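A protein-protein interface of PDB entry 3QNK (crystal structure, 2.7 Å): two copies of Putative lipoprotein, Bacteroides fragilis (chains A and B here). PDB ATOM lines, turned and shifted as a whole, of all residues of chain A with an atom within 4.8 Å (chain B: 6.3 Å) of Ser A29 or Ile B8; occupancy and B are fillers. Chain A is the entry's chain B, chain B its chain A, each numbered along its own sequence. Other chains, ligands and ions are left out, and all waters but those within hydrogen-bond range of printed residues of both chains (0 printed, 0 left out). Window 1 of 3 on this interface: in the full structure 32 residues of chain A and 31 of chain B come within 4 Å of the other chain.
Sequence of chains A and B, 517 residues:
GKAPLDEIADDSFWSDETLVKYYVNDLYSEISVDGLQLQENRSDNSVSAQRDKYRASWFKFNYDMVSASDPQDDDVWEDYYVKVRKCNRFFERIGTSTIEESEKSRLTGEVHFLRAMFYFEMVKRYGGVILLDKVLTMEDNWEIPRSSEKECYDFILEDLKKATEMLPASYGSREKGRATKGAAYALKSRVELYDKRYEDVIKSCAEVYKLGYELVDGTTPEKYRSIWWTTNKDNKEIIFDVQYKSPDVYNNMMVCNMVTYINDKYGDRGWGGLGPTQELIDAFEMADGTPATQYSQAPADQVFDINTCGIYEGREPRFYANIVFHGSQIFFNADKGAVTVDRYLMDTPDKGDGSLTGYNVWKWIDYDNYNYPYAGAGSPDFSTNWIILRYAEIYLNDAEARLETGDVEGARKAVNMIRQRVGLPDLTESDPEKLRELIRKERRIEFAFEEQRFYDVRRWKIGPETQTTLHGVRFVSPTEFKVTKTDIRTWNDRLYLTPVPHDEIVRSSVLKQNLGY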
ATOM      1  N   TYR A  22     -31.963  12.093 -28.750  1.00  0.00           N
ATOM      2  CA  TYR A  22     -30.519  12.232 -28.975  1.00  0.00           C
ATOM      3  C   TYR A  22     -29.749  12.242 -27.641  1.00  0.00           C
ATOM      4  O   TYR A  22     -28.653  11.683 -27.562  1.00  0.00           O
ATOM      5  CB  TYR A  22     -30.197  13.497 -29.785  1.00  0.00           C
ATOM      6  CG  TYR A  22     -30.503  13.407 -31.266  1.00  0.00           C
ATOM      7  CD1 TYR A  22     -30.588  12.173 -31.910  1.00  0.00           C
ATOM      8  CD2 TYR A  22     -30.652  14.556 -32.038  1.00  0.00           C
ATOM      9  CE1 TYR A  22     -30.893  12.084 -33.272  1.00  0.00           C
ATOM     10  CE2 TYR A  22     -30.933  14.483 -33.407  1.00  0.00           C
ATOM     11  CZ  TYR A  22     -31.056  13.243 -34.023  1.00  0.00           C
ATOM     12  OH  TYR A  22     -31.329  13.161 -35.377  1.00  0.00           O
ATOM     13  N   ASN A  25     -29.424   8.724 -26.555  1.00  0.00           N
ATOM     14  CA  ASN A  25     -28.402   8.095 -27.409  1.00  0.00           C
ATOM     15  C   ASN A  25     -27.007   8.412 -26.900  1.00  0.00           C
ATOM     16  O   ASN A  25     -26.135   7.533 -26.914  1.00  0.00           O
ATOM     17  CB  ASN A  25     -28.523   8.556 -28.865  1.00  0.00           C
ATOM     18  CG  ASN A  25     -29.725   8.061 -29.640  1.00  0.00           C
ATOM     19  OD1 ASN A  25     -30.652   7.411 -29.120  1.00  0.00           O
ATOM     20  ND2 ASN A  25     -29.731   8.382 -30.922  1.00  0.00           N
ATOM     21  N   ASP A  26     -26.807   9.666 -26.412  1.00  0.00           N
ATOM     22  CA  ASP A  26     -25.541  10.111 -25.831  1.00  0.00           C
ATOM     23  C   ASP A  26     -25.242   9.328 -24.564  1.00  0.00           C
ATOM     24  O   ASP A  26     -24.081   8.993 -24.313  1.00  0.00           O
ATOM     25  CB  ASP A  26     -25.578  11.614 -25.551  1.00  0.00           C
ATOM     26  CG  ASP A  26     -24.263  12.200 -25.076  1.00  0.00           C
ATOM     27  OD1 ASP A  26     -23.250  12.017 -25.779  1.00  0.00           O
ATOM     28  OD2 ASP A  26     -24.264  12.902 -24.027  1.00  0.00           O
ATOM     29  N   LEU A  27     -26.294   9.017 -23.772  1.00  0.00           N
ATOM     30  CA  LEU A  27     -26.144   8.253 -22.533  1.00  0.00           C
ATOM     31  C   LEU A  27     -25.749   6.816 -22.853  1.00  0.00           C
ATOM     32  O   LEU A  27     -24.905   6.250 -22.161  1.00  0.00           O
ATOM     33  CB  LEU A  27     -27.411   8.301 -21.665  1.00  0.00           C
ATOM     34  CG  LEU A  27     -27.802   9.653 -21.090  1.00  0.00           C
ATOM     35  CD1 LEU A  27     -29.193   9.609 -20.505  1.00  0.00           C
ATOM     36  CD2 LEU A  27     -26.857  10.079 -20.024  1.00  0.00           C
ATOM     37  N   TYR A  28     -26.307   6.246 -23.921  1.00  0.00           N
ATOM     38  CA  TYR A  28     -25.919   4.902 -24.353  1.00  0.00           C
ATOM     39  C   TYR A  28     -24.476   4.923 -24.845  1.00  0.00           C
ATOM     40  O   TYR A  28     -23.729   3.980 -24.588  1.00  0.00           O
ATOM     41  CB  TYR A  28     -26.841   4.379 -25.467  1.00  0.00           C
ATOM     42  CG  TYR A  28     -28.116   3.720 -24.991  1.00  0.00           C
ATOM     43  CD1 TYR A  28     -28.116   2.397 -24.538  1.00  0.00           C
ATOM     44  CD2 TYR A  28     -29.344   4.377 -25.085  1.00  0.00           C
ATOM     45  CE1 TYR A  28     -29.300   1.767 -24.141  1.00  0.00           C
ATOM     46  CE2 TYR A  28     -30.529   3.765 -24.673  1.00  0.00           C
ATOM     47  CZ  TYR A  28     -30.507   2.455 -24.213  1.00  0.00           C
ATOM     48  OH  TYR A  28     -31.677   1.848 -23.804  1.00  0.00           O
ATOM     49  N   SER A  29     -24.071   6.020 -25.522  1.00  0.00           N
ATOM     50  CA  SER A  29     -22.714   6.191 -26.055  1.00  0.00           C
ATOM     51  C   SER A  29     -21.675   6.263 -24.912  1.00  0.00           C
ATOM     52  O   SER A  29     -20.488   6.017 -25.142  1.00  0.00           O
ATOM     53  CB  SER A  29     -22.639   7.416 -26.970  1.00  0.00           C
ATOM     54  OG  SER A  29     -21.944   8.511 -26.395  1.00  0.00           O
ATOM     55  N   GLU A  30     -22.138   6.540 -23.679  1.00  0.00           N
ATOM     56  CA  GLU A  30     -21.283   6.590 -22.500  1.00  0.00           C
ATOM     57  C   GLU A  30     -20.924   5.188 -22.006  1.00  0.00           C
ATOM     58  O   GLU A  30     -20.100   5.072 -21.106  1.00  0.00           O
ATOM     59  CB  GLU A  30     -21.924   7.411 -21.373  1.00  0.00           C
ATOM     60  CG  GLU A  30     -21.858   8.915 -21.587  1.00  0.00           C
ATOM     61  CD  GLU A  30     -20.502   9.576 -21.715  1.00  0.00           C
ATOM     62  OE1 GLU A  30     -19.491   8.998 -21.253  1.00  0.00           O
ATOM     63  OE2 GLU A  30     -20.459  10.701 -22.262  1.00  0.00           O
ATOM     64  N   ILE A  31     -21.508   4.124 -22.589  1.00  0.00           N
ATOM     65  CA  ILE A  31     -21.143   2.760 -22.208  1.00  0.00           C
ATOM     66  C   ILE A  31     -19.721   2.528 -22.727  1.00  0.00           C
ATOM     67  O   ILE A  31     -19.467   2.689 -23.934  1.00  0.00           O
ATOM     68  CB  ILE A  31     -22.144   1.687 -22.724  1.00  0.00           C
ATOM     69  CG1 ILE A  31     -23.538   1.868 -22.122  1.00  0.00           C
ATOM     70  CG2 ILE A  31     -21.600   0.269 -22.454  1.00  0.00           C
ATOM     71  CD1 ILE A  31     -24.622   1.139 -22.916  1.00  0.00           C
ATOM     72  N   ALA B   3     -16.965  11.136 -28.745  1.00  0.00           N
ATOM     73  CA  ALA B   3     -17.320  10.977 -30.152  1.00  0.00           C
ATOM     74  C   ALA B   3     -17.844  12.292 -30.735  1.00  0.00           C
ATOM     75  O   ALA B   3     -18.474  13.074 -29.994  1.00  0.00           O
ATOM     76  CB  ALA B   3     -18.368   9.887 -30.305  1.00  0.00           C
ATOM     77  N   PRO B   4     -17.615  12.552 -32.057  1.00  0.00           N
ATOM     78  CA  PRO B   4     -18.198  13.758 -32.683  1.00  0.00           C
ATOM     79  C   PRO B   4     -19.729  13.710 -32.618  1.00  0.00           C
ATOM     80  O   PRO B   4     -20.299  12.622 -32.665  1.00  0.00           O
ATOM     81  CB  PRO B   4     -17.692  13.687 -34.126  1.00  0.00           C
ATOM     82  CG  PRO B   4     -16.513  12.768 -34.075  1.00  0.00           C
ATOM     83  CD  PRO B   4     -16.891  11.746 -33.061  1.00  0.00           C
ATOM     84  N   LEU B   5     -20.379  14.882 -32.481  1.00  0.00           N
ATOM     85  CA  LEU B   5     -21.824  15.032 -32.306  1.00  0.00           C
ATOM     86  C   LEU B   5     -22.665  14.249 -33.328  1.00  0.00           C
ATOM     87  O   LEU B   5     -23.679  13.675 -32.934  1.00  0.00           O
ATOM     88  CB  LEU B   5     -22.227  16.518 -32.337  1.00  0.00           C
ATOM     89  CG  LEU B   5     -23.623  16.841 -31.799  1.00  0.00           C
ATOM     90  CD1 LEU B   5     -23.606  16.957 -30.286  1.00  0.00           C
ATOM     91  CD2 LEU B   5     -24.161  18.112 -32.419  1.00  0.00           C
ATOM     92  N   ASP B   6     -22.237  14.197 -34.611  1.00  0.00           N
ATOM     93  CA  ASP B   6     -22.970  13.517 -35.688  1.00  0.00           C
ATOM     94  C   ASP B   6     -23.182  11.995 -35.436  1.00  0.00           C
ATOM     95  O   ASP B   6     -24.133  11.433 -35.988  1.00  0.00           O
ATOM     96  CB  ASP B   6     -22.314  13.764 -37.070  1.00  0.00           C
ATOM     97  CG  ASP B   6     -20.950  13.139 -37.342  1.00  0.00           C
ATOM     98  OD1 ASP B   6     -20.157  13.005 -36.390  1.00  0.00           O
ATOM     99  OD2 ASP B   6     -20.657  12.834 -38.524  1.00  0.00           O
ATOM    100  N   GLU B   7     -22.354  11.357 -34.572  1.00  0.00           N
ATOM    101  CA  GLU B   7     -22.444   9.923 -34.247  1.00  0.00           C
ATOM    102  C   GLU B   7     -23.723   9.578 -33.433  1.00  0.00           C
ATOM    103  O   GLU B   7     -24.179   8.434 -33.474  1.00  0.00           O
ATOM    104  CB  GLU B   7     -21.179   9.449 -33.509  1.00  0.00           C
ATOM    105  CG  GLU B   7     -19.899   9.641 -34.310  1.00  0.00           C
ATOM    106  CD  GLU B   7     -18.945   8.464 -34.347  1.00  0.00           C
ATOM    107  OE1 GLU B   7     -19.415   7.333 -34.605  1.00  0.00           O
ATOM    108  OE2 GLU B   7     -17.720   8.677 -34.193  1.00  0.00           O
ATOM    109  N   ILE B   8     -24.311  10.565 -32.738  1.00  0.00           N
ATOM    110  CA  ILE B   8     -25.523  10.440 -31.920  1.00  0.00           C
ATOM    111  C   ILE B   8     -26.789  10.495 -32.810  1.00  0.00           C
ATOM    112  O   ILE B   8     -27.806   9.889 -32.467  1.00  0.00           O
ATOM    113  CB  ILE B   8     -25.507  11.591 -30.844  1.00  0.00           C
ATOM    114  CG1 ILE B   8     -24.294  11.505 -29.895  1.00  0.00           C
ATOM    115  CG2 ILE B   8     -26.812  11.745 -30.064  1.00  0.00           C
ATOM    116  CD1 ILE B   8     -24.101  10.142 -29.142  1.00  0.00           C
ATOM    117  N   ALA B   9     -26.713  11.217 -33.948  1.00  0.00           N
ATOM    118  CA  ALA B   9     -27.839  11.455 -34.857  1.00  0.00           C
ATOM    119  C   ALA B   9     -27.901  10.537 -36.082  1.00  0.00           C
ATOM    120  O   ALA B   9     -26.960   9.786 -36.372  1.00  0.00           O
ATOM    121  CB  ALA B   9     -27.825  12.902 -35.325  1.00  0.00           C
ATOM    122  N   ASP B  10     -29.061  10.640 -36.798  1.00  0.00           N
ATOM    123  CA  ASP B  10     -29.460   9.950 -38.026  1.00  0.00           C
ATOM    124  C   ASP B  10     -28.593  10.370 -39.219  1.00  0.00           C
ATOM    125  O   ASP B  10     -28.042  11.478 -39.226  1.00  0.00           O
ATOM    126  CB  ASP B  10     -30.938  10.253 -38.336  1.00  0.00           C
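O of Asp A26 is in hydrogen-bond range of OG of Ser A29 (3.0 Å).
Of the printed residues of chain B, Tyr A22 touches Ile B8, Ala B9 and Asp B10.
Printed residues of chain B within 4 Å of Asn A25: Ile B8 (2.9 Å).
Of the printed residues of chain B, Asp A26 touches Ile B8 (3.6 Å).
Leu A27 touches none of the printed residues of chain B.
Ser A29 touches just one residue of chain B: Ile B8.
Asp B6 touches none of the printed residues of chain A.
Ile B8 touches just these residues of chain A: Tyr A22 (3.1 Å), Asn A25 (2.9 Å), Asp A26 (3.6 Å) and Ser A29 (3.8 Å).
Of the printed residues of chain A, Asp B10 touches Tyr A22 (3.7 Å).
The nearest printed residue of chain A that does not touch Ala B9 is Asn A25 (5.1 Å).
No position is printed for both chains.
Among the printed residues, merely in contact across the chains: Tyr A22 with Ile B8 (3.1 Å), Tyr A22 with Ala B9 (3.5 Å), Tyr A22 with Asp B10 (3.7 Å), Asp A26 with Ile B8 (3.6 Å) and Ser A29 with Ile B8 (3.8 Å).
The side-chain amide nitrogen (ND2) of Asn A25 lies within hydrogen-bond range of the backbone carbonyl oxygen (O) of Ile B8, at 2.9 Å.
Of the 8 printed residues of chain B, 3 touch a printed residue of chain A.
Hydrophobic or aromatic side chains of chain A within 4 Å of the printed part of chain B: Tyr A22.
Among the printed residues, 6 pairs touch across the chains.
Among the printed residues, no Asp or Glu carboxylate lies within 4 Å of a Lys or Arg side-chain nitrogen of the other chain.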
